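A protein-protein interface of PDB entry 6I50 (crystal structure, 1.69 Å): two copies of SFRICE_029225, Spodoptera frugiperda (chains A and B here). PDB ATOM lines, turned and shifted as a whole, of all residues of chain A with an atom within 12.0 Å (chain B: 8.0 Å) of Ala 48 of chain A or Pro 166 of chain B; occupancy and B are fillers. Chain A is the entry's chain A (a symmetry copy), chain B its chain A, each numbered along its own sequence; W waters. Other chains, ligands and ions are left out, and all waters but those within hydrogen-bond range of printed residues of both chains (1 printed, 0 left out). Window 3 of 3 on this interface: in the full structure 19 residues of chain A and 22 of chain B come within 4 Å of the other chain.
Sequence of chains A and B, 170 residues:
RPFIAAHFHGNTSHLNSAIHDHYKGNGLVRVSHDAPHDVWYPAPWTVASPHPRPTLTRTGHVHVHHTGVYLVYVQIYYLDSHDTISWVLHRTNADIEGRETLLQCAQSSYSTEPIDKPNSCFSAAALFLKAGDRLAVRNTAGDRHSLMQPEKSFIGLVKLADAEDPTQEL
A ring nitrogen (ND1) of His 51 of chain A lies within hydrogen-bond range of the backbone NH of Phe 3 of chain A, at 3.4 Å.
The backbone NH (N) of Thr 167 of chain B is in hydrogen-bond range of the side-chain carboxylate (OD1) of Asp 165 of chain B.
CE2 of Phe 3 of chain A touches CG1 of Val 69 of chain B (3.97 Å).
O of Pro 44 of chain A touches CB of Pro 166 of chain B (3.4 Å).
CG2 of Thr 167 of chain B touches CB of Pro 44 of chain A, at 3.7 Å.
Trp 45 of chain A touches Val 69 of chain B (CD2 to CG2, 3.7 Å).
N of Phe 128 of chain B touches CD1 of Trp 45 of chain A (3.9 Å).
Trp 45 of chain A touches Pro 166 of chain B.
Ala 48 of chain A touches Pro 166 of chain B (CB to CB, 3.7 Å).
Of the printed residues of chain B, Trp 45 of chain A touches Val 69, Phe 128 and Pro 166.
Ala 48 of chain A touches just one residue of chain B: Pro 166.
Pro 52 of chain A touches none of the printed residues of chain B.
Thr 67 of chain B touches none of the printed residues of chain A.
Printed residues of chain A within 4 Å of Val 69 of chain B: Phe 3 (3.97 Å) and Trp 45 (3.7 Å).
No residue of chain A comes within 4 Å of Asp 165 of chain B.
Pro 166 of chain B touches just these residues of chain A: Pro 44 (3.4 Å), Trp 45 (3.7 Å) and Ala 48 (3.7 Å).
Printed residues of chain A within 4 Å of Thr 167 of chain B: Pro 44 (3.7 Å).
No residue of chain A comes within 4 Å of Gln 168 of chain B.
Of the 13 printed residues of chain B, 4 touch a printed residue of chain A.
Printed residues of chain B that touch a printed residue of chain A: Val 69, Phe 128, Pro 166 and Thr 167.
Of the 23 printed residues of chain A, 4 touch a printed residue of chain B.
No position is printed for both chains.
Of the 7 pairs that touch across the chains among the printed residues, none has its exchanged pair printed and touching as well.
Water W1 bridges the backbone carbonyl oxygen (O) of Pro 166 of chain B (2.8 Å) and the backbone carbonyl oxygen (O) of Pro 44 of chain A (2.8 Å).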
ATOM      1  N   PHE A   3     -30.103 -18.594 -20.606  1.00  0.00           N
ATOM      2  CA  PHE A   3     -30.689 -19.271 -19.450  1.00  0.00           C
ATOM      3  C   PHE A   3     -30.275 -18.470 -18.221  1.00  0.00           C
ATOM      4  O   PHE A   3     -29.235 -18.719 -17.614  1.00  0.00           O
ATOM      5  CB  PHE A   3     -30.213 -20.718 -19.383  1.00  0.00           C
ATOM      6  CG  PHE A   3     -30.860 -21.533 -18.295  1.00  0.00           C
ATOM      7  CD1 PHE A   3     -32.230 -21.486 -18.091  1.00  0.00           C
ATOM      8  CD2 PHE A   3     -30.100 -22.383 -17.510  1.00  0.00           C
ATOM      9  CE1 PHE A   3     -32.826 -22.258 -17.107  1.00  0.00           C
ATOM     10  CE2 PHE A   3     -30.685 -23.153 -16.521  1.00  0.00           C
ATOM     11  CZ  PHE A   3     -32.049 -23.094 -16.321  1.00  0.00           C
ATOM     12  N   ILE A   4     -31.091 -17.478 -17.868  1.00  0.00           N
ATOM     13  CA  ILE A   4     -30.792 -16.581 -16.747  1.00  0.00           C
ATOM     14  C   ILE A   4     -31.335 -17.266 -15.495  1.00  0.00           C
ATOM     15  O   ILE A   4     -32.483 -17.070 -15.099  1.00  0.00           O
ATOM     16  CB  ILE A   4     -31.372 -15.187 -16.969  1.00  0.00           C
ATOM     17  CG1 ILE A   4     -30.809 -14.607 -18.273  1.00  0.00           C
ATOM     18  CG2 ILE A   4     -31.059 -14.268 -15.789  1.00  0.00           C
ATOM     19  CD1 ILE A   4     -31.248 -13.201 -18.558  1.00  0.00           C
ATOM     20  N   ALA A   5     -30.494 -18.086 -14.865  1.00  0.00           N
ATOM     21  CA  ALA A   5     -30.952 -18.989 -13.822  1.00  0.00           C
ATOM     22  C   ALA A   5     -29.761 -19.415 -12.979  1.00  0.00           C
ATOM     23  O   ALA A   5     -28.625 -19.426 -13.454  1.00  0.00           O
ATOM     24  CB  ALA A   5     -31.642 -20.221 -14.417  1.00  0.00           C
ATOM     25  N   ALA A   6     -30.037 -19.781 -11.733  1.00  0.00           N
ATOM     26  CA  ALA A   6     -28.994 -20.225 -10.819  1.00  0.00           C
ATOM     27  C   ALA A   6     -29.628 -21.044  -9.702  1.00  0.00           C
ATOM     28  O   ALA A   6     -30.780 -20.822  -9.322  1.00  0.00           O
ATOM     29  CB  ALA A   6     -28.211 -19.038 -10.238  1.00  0.00           C
ATOM     30  N   HIS A   7     -28.854 -21.997  -9.185  1.00  0.00           N
ATOM     31  CA  HIS A   7     -29.259 -22.814  -8.050  1.00  0.00           C
ATOM     32  C   HIS A   7     -28.122 -22.813  -7.042  1.00  0.00           C
ATOM     33  O   HIS A   7     -26.977 -23.086  -7.406  1.00  0.00           O
ATOM     34  CB  HIS A   7     -29.581 -24.249  -8.475  1.00  0.00           C
ATOM     35  CG  HIS A   7     -30.012 -25.129  -7.344  1.00  0.00           C
ATOM     36  ND1 HIS A   7     -31.325 -25.219  -6.930  1.00  0.00           N
ATOM     37  CD2 HIS A   7     -29.306 -25.954  -6.535  1.00  0.00           C
ATOM     38  CE1 HIS A   7     -31.409 -26.073  -5.924  1.00  0.00           C
ATOM     39  NE2 HIS A   7     -30.198 -26.535  -5.668  1.00  0.00           N
ATOM     40  N   PHE A   8     -28.428 -22.473  -5.795  1.00  0.00           N
ATOM     41  CA  PHE A   8     -27.447 -22.452  -4.715  1.00  0.00           C
ATOM     42  C   PHE A   8     -27.929 -23.391  -3.622  1.00  0.00           C
ATOM     43  O   PHE A   8     -29.100 -23.339  -3.232  1.00  0.00           O
ATOM     44  CB  PHE A   8     -27.268 -21.036  -4.161  1.00  0.00           C
ATOM     45  CG  PHE A   8     -27.045 -20.005  -5.221  1.00  0.00           C
ATOM     46  CD1 PHE A   8     -25.775 -19.793  -5.733  1.00  0.00           C
ATOM     47  CD2 PHE A   8     -28.107 -19.270  -5.731  1.00  0.00           C
ATOM     48  CE1 PHE A   8     -25.558 -18.848  -6.723  1.00  0.00           C
ATOM     49  CE2 PHE A   8     -27.900 -18.319  -6.718  1.00  0.00           C
ATOM     50  CZ  PHE A   8     -26.620 -18.117  -7.219  1.00  0.00           C
ATOM     51  N   HIS A   9     -27.041 -24.244  -3.119  1.00  0.00           N
ATOM     52  CA  HIS A   9     -27.472 -25.224  -2.134  1.00  0.00           C
ATOM     53  C   HIS A   9     -26.558 -25.201  -0.916  1.00  0.00           C
ATOM     54  O   HIS A   9     -25.470 -24.617  -0.932  1.00  0.00           O
ATOM     55  CB  HIS A   9     -27.562 -26.647  -2.734  1.00  0.00           C
ATOM     56  CG  HIS A   9     -26.303 -27.129  -3.388  1.00  0.00           C
ATOM     57  ND1 HIS A   9     -26.318 -27.944  -4.501  1.00  0.00           N
ATOM     58  CD2 HIS A   9     -24.999 -26.949  -3.072  1.00  0.00           C
ATOM     59  CE1 HIS A   9     -25.078 -28.229  -4.854  1.00  0.00           C
ATOM     60  NE2 HIS A   9     -24.257 -27.640  -4.002  1.00  0.00           N
ATOM     61  N   TYR A  41     -23.833 -22.320  -1.672  1.00  0.00           N
ATOM     62  CA  TYR A  41     -22.794 -22.444  -2.674  1.00  0.00           C
ATOM     63  C   TYR A  41     -23.464 -22.826  -3.985  1.00  0.00           C
ATOM     64  O   TYR A  41     -24.394 -23.644  -3.977  1.00  0.00           O
ATOM     65  CB  TYR A  41     -21.742 -23.495  -2.294  1.00  0.00           C
ATOM     66  CG  TYR A  41     -20.469 -23.369  -3.094  1.00  0.00           C
ATOM     67  CD1 TYR A  41     -19.459 -22.509  -2.687  1.00  0.00           C
ATOM     68  CD2 TYR A  41     -20.282 -24.100  -4.259  1.00  0.00           C
ATOM     69  CE1 TYR A  41     -18.293 -22.380  -3.419  1.00  0.00           C
ATOM     70  CE2 TYR A  41     -19.118 -23.977  -5.000  1.00  0.00           C
ATOM     71  CZ  TYR A  41     -18.128 -23.114  -4.573  1.00  0.00           C
ATOM     72  OH  TYR A  41     -16.966 -22.984  -5.300  1.00  0.00           O
ATOM     73  N   PRO A  42     -23.027 -22.265  -5.110  1.00  0.00           N
ATOM     74  CA  PRO A  42     -23.642 -22.629  -6.395  1.00  0.00           C
ATOM     75  C   PRO A  42     -23.477 -24.111  -6.709  1.00  0.00           C
ATOM     76  O   PRO A  42     -22.414 -24.702  -6.488  1.00  0.00           O
ATOM     77  CB  PRO A  42     -22.889 -21.754  -7.407  1.00  0.00           C
ATOM     78  CG  PRO A  42     -21.604 -21.396  -6.724  1.00  0.00           C
ATOM     79  CD  PRO A  42     -21.960 -21.266  -5.275  1.00  0.00           C
ATOM     80  N   ALA A  43     -24.558 -24.715  -7.216  1.00  0.00           N
ATOM     81  CA  ALA A  43     -24.489 -26.070  -7.736  1.00  0.00           C
ATOM     82  C   ALA A  43     -23.528 -26.113  -8.924  1.00  0.00           C
ATOM     83  O   ALA A  43     -23.261 -25.085  -9.554  1.00  0.00           O
ATOM     84  CB  ALA A  43     -25.877 -26.552  -8.154  1.00  0.00           C
ATOM     85  N   PRO A  44     -22.990 -27.289  -9.249  1.00  0.00           N
ATOM     86  CA  PRO A  44     -22.016 -27.357 -10.351  1.00  0.00           C
ATOM     87  C   PRO A  44     -22.524 -26.782 -11.665  1.00  0.00           C
ATOM     88  O   PRO A  44     -21.760 -26.104 -12.361  1.00  0.00           O
ATOM     89  CB  PRO A  44     -21.720 -28.859 -10.445  1.00  0.00           C
ATOM     90  CG  PRO A  44     -21.881 -29.338  -9.041  1.00  0.00           C
ATOM     91  CD  PRO A  44     -23.051 -28.553  -8.490  1.00  0.00           C
ATOM     92  N   TRP A  45     -23.789 -27.019 -12.026  1.00  0.00           N
ATOM     93  CA  TRP A  45     -24.265 -26.490 -13.300  1.00  0.00           C
ATOM     94  C   TRP A  45     -24.303 -24.969 -13.284  1.00  0.00           C
ATOM     95  O   TRP A  45     -24.140 -24.334 -14.331  1.00  0.00           O
ATOM     96  CB  TRP A  45     -25.638 -27.076 -13.660  1.00  0.00           C
ATOM     97  CG  TRP A  45     -26.846 -26.565 -12.904  1.00  0.00           C
ATOM     98  CD1 TRP A  45     -27.522 -27.215 -11.908  1.00  0.00           C
ATOM     99  CD2 TRP A  45     -27.556 -25.334 -13.129  1.00  0.00           C
ATOM    100  NE1 TRP A  45     -28.592 -26.457 -11.482  1.00  0.00           N
ATOM    101  CE2 TRP A  45     -28.634 -25.298 -12.215  1.00  0.00           C
ATOM    102  CE3 TRP A  45     -27.382 -24.258 -14.008  1.00  0.00           C
ATOM    103  CZ2 TRP A  45     -29.529 -24.226 -12.153  1.00  0.00           C
ATOM    104  CZ3 TRP A  45     -28.266 -23.192 -13.942  1.00  0.00           C
ATOM    105  CH2 TRP A  45     -29.327 -23.185 -13.021  1.00  0.00           C
ATOM    106  N   THR A  46     -24.495 -24.375 -12.109  1.00  0.00           N
ATOM    107  CA  THR A  46     -24.458 -22.924 -11.990  1.00  0.00           C
ATOM    108  C   THR A  46     -23.032 -22.401 -12.108  1.00  0.00           C
ATOM    109  O   THR A  46     -22.778 -21.433 -12.831  1.00  0.00           O
ATOM    110  CB  THR A  46     -25.099 -22.511 -10.663  1.00  0.00           C
ATOM    111  OG1 THR A  46     -26.482 -22.883 -10.688  1.00  0.00           O
ATOM    112  CG2 THR A  46     -24.974 -21.019 -10.443  1.00  0.00           C
ATOM    113  N   VAL A  47     -22.082 -23.044 -11.423  1.00  0.00           N
ATOM    114  CA  VAL A  47     -20.672 -22.666 -11.554  1.00  0.00           C
ATOM    115  C   VAL A  47     -20.234 -22.705 -13.013  1.00  0.00           C
ATOM    116  O   VAL A  47     -19.514 -21.817 -13.490  1.00  0.00           O
ATOM    117  CB  VAL A  47     -19.790 -23.585 -10.687  1.00  0.00           C
ATOM    118  CG1 VAL A  47     -18.305 -23.394 -11.024  1.00  0.00           C
ATOM    119  CG2 VAL A  47     -20.039 -23.331  -9.206  1.00  0.00           C
ATOM    120  N   ALA A  48     -20.659 -23.736 -13.743  1.00  0.00           N
ATOM    121  CA  ALA A  48     -20.237 -23.972 -15.117  1.00  0.00           C
ATOM    122  C   ALA A  48     -21.086 -23.248 -16.156  1.00  0.00           C
ATOM    123  O   ALA A  48     -20.773 -23.324 -17.350  1.00  0.00           O
ATOM    124  CB  ALA A  48     -20.258 -25.473 -15.414  1.00  0.00           C
ATOM    125  N   SER A  49     -22.133 -22.546 -15.747  1.00  0.00           N
ATOM    126  CA  SER A  49     -23.061 -21.972 -16.714  1.00  0.00           C
ATOM    127  C   SER A  49     -22.379 -20.892 -17.551  1.00  0.00           C
ATOM    128  O   SER A  49     -21.755 -19.980 -16.993  1.00  0.00           O
ATOM    129  CB  SER A  49     -24.272 -21.379 -15.999  1.00  0.00           C
ATOM    130  OG  SER A  49     -25.083 -20.677 -16.924  1.00  0.00           O
ATOM    131  N   PRO A  50     -22.479 -20.950 -18.882  1.00  0.00           N
ATOM    132  CA  PRO A  50     -21.954 -19.866 -19.720  1.00  0.00           C
ATOM    133  C   PRO A  50     -22.860 -18.649 -19.808  1.00  0.00           C
ATOM    134  O   PRO A  50     -22.521 -17.702 -20.525  1.00  0.00           O
ATOM    135  CB  PRO A  50     -21.823 -20.544 -21.089  1.00  0.00           C
ATOM    136  CG  PRO A  50     -22.953 -21.522 -21.101  1.00  0.00           C
ATOM    137  CD  PRO A  50     -23.055 -22.042 -19.686  1.00  0.00           C
ATOM    138  N   HIS A  51     -24.001 -18.635 -19.097  1.00  0.00           N
ATOM    139  CA  HIS A  51     -25.015 -17.603 -19.254  1.00  0.00           C
ATOM    140  C   HIS A  51     -24.873 -16.518 -18.194  1.00  0.00           C
ATOM    141  O   HIS A  51     -24.432 -16.787 -17.074  1.00  0.00           O
ATOM    142  CB  HIS A  51     -26.422 -18.205 -19.142  1.00  0.00           C
ATOM    143  CG  HIS A  51     -26.653 -19.377 -20.047  1.00  0.00           C
ATOM    144  ND1 HIS A  51     -26.902 -19.238 -21.395  1.00  0.00           N
ATOM    145  CD2 HIS A  51     -26.668 -20.708 -19.795  1.00  0.00           C
ATOM    146  CE1 HIS A  51     -27.065 -20.435 -21.934  1.00  0.00           C
ATOM    147  NE2 HIS A  51     -26.926 -21.343 -20.984  1.00  0.00           N
ATOM    148  N   PRO A  52     -25.253 -15.283 -18.520  1.00  0.00           N
ATOM    149  CA  PRO A  52     -25.495 -14.294 -17.463  1.00  0.00           C
ATOM    150  C   PRO A  52     -26.569 -14.828 -16.530  1.00  0.00           C
ATOM    151  O   PRO A  52     -27.515 -15.486 -16.969  1.00  0.00           O
ATOM    152  CB  PRO A  52     -25.973 -13.051 -18.227  1.00  0.00           C
ATOM    153  CG  PRO A  52     -25.587 -13.283 -19.655  1.00  0.00           C
ATOM    154  CD  PRO A  52     -25.571 -14.767 -19.861  1.00  0.00           C
ATOM    155  N   ARG A  53     -26.416 -14.563 -15.237  1.00  0.00           N
ATOM    156  CA  ARG A  53     -27.255 -15.243 -14.257  1.00  0.00           C
ATOM    157  C   ARG A  53     -27.154 -14.514 -12.928  1.00  0.00           C
ATOM    158  O   ARG A  53     -26.211 -13.747 -12.706  1.00  0.00           O
ATOM    159  CB  ARG A  53     -26.818 -16.705 -14.084  1.00  0.00           C
ATOM    160  CG  ARG A  53     -25.366 -16.848 -13.636  1.00  0.00           C
ATOM    161  CD  ARG A  53     -25.168 -18.162 -12.914  1.00  0.00           C
ATOM    162  NE  ARG A  53     -23.761 -18.491 -12.669  1.00  0.00           N
ATOM    163  CZ  ARG A  53     -23.128 -18.284 -11.515  1.00  0.00           C
ATOM    164  NH1 ARG A  53     -23.766 -17.731 -10.490  1.00  0.00           N
ATOM    165  NH2 ARG A  53     -21.856 -18.643 -11.387  1.00  0.00           N
ATOM    166  N   PRO A  54     -28.095 -14.752 -12.012  1.00  0.00           N
ATOM    167  CA  PRO A  54     -27.916 -14.279 -10.636  1.00  0.00           C
ATOM    168  C   PRO A  54     -26.667 -14.886 -10.017  1.00  0.00           C
ATOM    169  O   PRO A  54     -26.254 -15.996 -10.358  1.00  0.00           O
ATOM    170  CB  PRO A  54     -29.184 -14.767  -9.920  1.00  0.00           C
ATOM    171  CG  PRO A  54     -30.173 -15.009 -11.016  1.00  0.00           C
ATOM    172  CD  PRO A  54     -29.368 -15.466 -12.195  1.00  0.00           C
ATOM    173  N   THR A  55     -26.075 -14.155  -9.078  1.00  0.00           N
ATOM    174  CA  THR A  55     -24.840 -14.584  -8.440  1.00  0.00           C
ATOM    175  C   THR A  55     -25.015 -14.563  -6.927  1.00  0.00           C
ATOM    176  O   THR A  55     -26.003 -14.046  -6.401  1.00  0.00           O
ATOM    177  CB  THR A  55     -23.646 -13.711  -8.867  1.00  0.00           C
ATOM    178  OG1 THR A  55     -23.921 -12.332  -8.573  1.00  0.00           O
ATOM    179  CG2 THR A  55     -23.379 -13.868 -10.366  1.00  0.00           C
ATOM    180  N   LEU A  56     -24.041 -15.143  -6.229  1.00  0.00           N
ATOM    181  CA  LEU A  56     -24.088 -15.300  -4.779  1.00  0.00           C
ATOM    182  C   LEU A  56     -23.036 -14.410  -4.132  1.00  0.00           C
ATOM    183  O   LEU A  56     -21.847 -14.501  -4.464  1.00  0.00           O
ATOM    184  CB  LEU A  56     -23.864 -16.762  -4.379  1.00  0.00           C
ATOM    185  CG  LEU A  56     -23.940 -17.095  -2.886  1.00  0.00           C
ATOM    186  CD1 LEU A  56     -25.364 -16.913  -2.388  1.00  0.00           C
ATOM    187  CD2 LEU A  56     -23.435 -18.517  -2.628  1.00  0.00           C
ATOM    188  N   THR B  67     -29.627 -34.726 -21.951  1.00  0.00           N
ATOM    189  CA  THR B  67     -28.849 -34.019 -20.944  1.00  0.00           C
ATOM    190  C   THR B  67     -29.276 -32.557 -20.857  1.00  0.00           C
ATOM    191  O   THR B  67     -29.496 -31.898 -21.877  1.00  0.00           O
ATOM    192  CB  THR B  67     -27.364 -34.114 -21.291  1.00  0.00           C
ATOM    193  OG1 THR B  67     -26.972 -35.494 -21.317  1.00  0.00           O
ATOM    194  CG2 THR B  67     -26.520 -33.362 -20.274  1.00  0.00           C
ATOM    195  N   GLY B  68     -29.402 -32.051 -19.636  1.00  0.00           N
ATOM    196  CA  GLY B  68     -29.696 -30.643 -19.460  1.00  0.00           C
ATOM    197  C   GLY B  68     -30.037 -30.333 -18.021  1.00  0.00           C
ATOM    198  O   GLY B  68     -29.940 -31.183 -17.131  1.00  0.00           O
ATOM    199  N   VAL B  69     -30.421 -29.079 -17.805  1.00  0.00           N
ATOM    200  CA  VAL B  69     -30.921 -28.644 -16.504  1.00  0.00           C
ATOM    201  C   VAL B  69     -32.435 -28.762 -16.532  1.00  0.00           C
ATOM    202  O   VAL B  69     -33.092 -28.188 -17.409  1.00  0.00           O
ATOM    203  CB  VAL B  69     -30.478 -27.212 -16.174  1.00  0.00           C
ATOM    204  CG1 VAL B  69     -31.114 -26.742 -14.870  1.00  0.00           C
ATOM    205  CG2 VAL B  69     -28.967 -27.150 -16.071  1.00  0.00           C
ATOM    206  N   PHE B 128     -29.177 -30.711 -12.657  1.00  0.00           N
ATOM    207  CA  PHE B 128     -28.518 -31.183 -13.862  1.00  0.00           C
ATOM    208  C   PHE B 128     -28.713 -32.687 -13.973  1.00  0.00           C
ATOM    209  O   PHE B 128     -28.384 -33.431 -13.046  1.00  0.00           O
ATOM    210  CB  PHE B 128     -27.029 -30.847 -13.856  1.00  0.00           C
ATOM    211  CG  PHE B 128     -26.287 -31.470 -14.995  1.00  0.00           C
ATOM    212  CD1 PHE B 128     -26.298 -30.877 -16.252  1.00  0.00           C
ATOM    213  CD2 PHE B 128     -25.623 -32.679 -14.829  1.00  0.00           C
ATOM    214  CE1 PHE B 128     -25.641 -31.468 -17.315  1.00  0.00           C
ATOM    215  CE2 PHE B 128     -24.960 -33.268 -15.886  1.00  0.00           C
ATOM    216  CZ  PHE B 128     -24.970 -32.665 -17.128  1.00  0.00           C
ATOM    217  N   LEU B 129     -29.241 -33.132 -15.111  1.00  0.00           N
ATOM    218  CA  LEU B 129     -29.454 -34.550 -15.371  1.00  0.00           C
ATOM    219  C   LEU B 129     -28.802 -34.924 -16.692  1.00  0.00           C
ATOM    220  O   LEU B 129     -28.811 -34.135 -17.643  1.00  0.00           O
ATOM    221  CB  LEU B 129     -30.945 -34.894 -15.419  1.00  0.00           C
ATOM    222  CG  LEU B 129     -31.758 -34.500 -14.180  1.00  0.00           C
ATOM    223  CD1 LEU B 129     -33.236 -34.754 -14.407  1.00  0.00           C
ATOM    224  CD2 LEU B 129     -31.275 -35.258 -12.954  1.00  0.00           C
ATOM    225  N   LYS B 130     -28.232 -36.126 -16.748  1.00  0.00           N
ATOM    226  CA  LYS B 130     -27.602 -36.638 -17.958  1.00  0.00           C
ATOM    227  C   LYS B 130     -28.513 -37.634 -18.664  1.00  0.00           C
ATOM    228  O   LYS B 130     -29.245 -38.394 -18.027  1.00  0.00           O
ATOM    229  CB  LYS B 130     -26.275 -37.337 -17.645  1.00  0.00           C
ATOM    230  CG  LYS B 130     -25.208 -36.448 -17.061  1.00  0.00           C
ATOM    231  CD  LYS B 130     -23.843 -37.120 -17.117  1.00  0.00           C
ATOM    232  CE  LYS B 130     -23.354 -37.257 -18.547  1.00  0.00           C
ATOM    233  NZ  LYS B 130     -21.869 -37.351 -18.602  1.00  0.00           N
ATOM    234  N   ALA B 163     -27.168 -28.111 -21.372  1.00  0.00           N
ATOM    235  CA  ALA B 163     -26.015 -27.928 -20.504  1.00  0.00           C
ATOM    236  C   ALA B 163     -25.015 -29.044 -20.758  1.00  0.00           C
ATOM    237  O   ALA B 163     -25.403 -30.203 -20.922  1.00  0.00           O
ATOM    238  CB  ALA B 163     -26.424 -27.914 -19.024  1.00  0.00           C
ATOM    239  N   GLU B 164     -23.735 -28.687 -20.790  1.00  0.00           N
ATOM    240  CA  GLU B 164     -22.674 -29.676 -20.760  1.00  0.00           C
ATOM    241  C   GLU B 164     -22.511 -30.214 -19.340  1.00  0.00           C
ATOM    242  O   GLU B 164     -22.922 -29.583 -18.364  1.00  0.00           O
ATOM    243  CB  GLU B 164     -21.362 -29.062 -21.241  1.00  0.00           C
ATOM    244  CG  GLU B 164     -21.496 -28.260 -22.519  1.00  0.00           C
ATOM    245  CD  GLU B 164     -20.977 -29.012 -23.725  1.00  0.00           C
ATOM    246  OE1 GLU B 164     -20.087 -29.874 -23.552  1.00  0.00           O
ATOM    247  OE2 GLU B 164     -21.457 -28.743 -24.845  1.00  0.00           O
ATOM    248  N   ASP B 165     -21.911 -31.396 -19.232  1.00  0.00           N
ATOM    249  CA  ASP B 165     -21.606 -31.961 -17.920  1.00  0.00           C
ATOM    250  C   ASP B 165     -20.762 -30.978 -17.116  1.00  0.00           C
ATOM    251  O   ASP B 165     -19.644 -30.648 -17.535  1.00  0.00           O
ATOM    252  CB  ASP B 165     -20.870 -33.292 -18.065  1.00  0.00           C
ATOM    253  CG  ASP B 165     -20.870 -34.108 -16.780  1.00  0.00           C
ATOM    254  OD1 ASP B 165     -20.816 -33.516 -15.677  1.00  0.00           O
ATOM    255  OD2 ASP B 165     -20.930 -35.350 -16.872  1.00  0.00           O
ATOM    256  N   PRO B 166     -21.244 -30.484 -15.972  1.00  0.00           N
ATOM    257  CA  PRO B 166     -20.501 -29.468 -15.217  1.00  0.00           C
ATOM    258  C   PRO B 166     -19.452 -30.016 -14.264  1.00  0.00           C
ATOM    259  O   PRO B 166     -18.730 -29.222 -13.653  1.00  0.00           O
ATOM    260  CB  PRO B 166     -21.616 -28.770 -14.430  1.00  0.00           C
ATOM    261  CG  PRO B 166     -22.586 -29.860 -14.153  1.00  0.00           C
ATOM    262  CD  PRO B 166     -22.550 -30.780 -15.357  1.00  0.00           C
ATOM    263  N   THR B 167     -19.362 -31.331 -14.108  1.00  0.00           N
ATOM    264  CA  THR B 167     -18.376 -31.950 -13.241  1.00  0.00           C
ATOM    265  C   THR B 167     -17.442 -32.809 -14.077  1.00  0.00           C
ATOM    266  O   THR B 167     -17.811 -33.307 -15.144  1.00  0.00           O
ATOM    267  CB  THR B 167     -19.032 -32.813 -12.157  1.00  0.00           C
ATOM    268  OG1 THR B 167     -19.698 -33.926 -12.767  1.00  0.00           O
ATOM    269  CG2 THR B 167     -20.040 -31.992 -11.349  1.00  0.00           C
ATOM    270  N   GLN B 168     -16.220 -32.968 -13.592  1.00  0.00           N
ATOM    271  CA  GLN B 168     -15.303 -33.921 -14.189  1.00  0.00           C
ATOM    272  C   GLN B 168     -14.635 -34.690 -13.064  1.00  0.00           C
ATOM    273  O   GLN B 168     -14.587 -34.239 -11.917  1.00  0.00           O
ATOM    274  CB  GLN B 168     -14.267 -33.236 -15.088  1.00  0.00           C
ATOM    275  CG  GLN B 168     -13.321 -32.309 -14.361  1.00  0.00           C
ATOM    276  CD  GLN B 168     -12.454 -31.516 -15.317  1.00  0.00           C
ATOM    277  OE1 GLN B 168     -12.906 -31.101 -16.385  1.00  0.00           O
ATOM    278  NE2 GLN B 168     -11.196 -31.307 -14.941  1.00  0.00           N
ATOM    279  N   GLU B 169     -14.146 -35.875 -13.400  1.00  0.00           N
ATOM    280  CA  GLU B 169     -13.442 -36.673 -12.417  1.00  0.00           C
ATOM    281  C   GLU B 169     -12.078 -36.050 -12.134  1.00  0.00           C
ATOM    282  O   GLU B 169     -11.590 -35.198 -12.878  1.00  0.00           O
ATOM    283  CB  GLU B 169     -13.318 -38.115 -12.904  1.00  0.00           C
ATOM    284  CG  GLU B 169     -14.683 -38.742 -13.178  1.00  0.00           C
ATOM    285  CD  GLU B 169     -14.592 -40.105 -13.827  1.00  0.00           C
ATOM    286  OE1 GLU B 169     -13.510 -40.451 -14.338  1.00  0.00           O
ATOM    287  OE2 GLU B 169     -15.608 -40.829 -13.830  1.00  0.00           O
HETATM  288  O   HOH W   1     -19.024 -26.816 -12.270  1.00  0.00           O
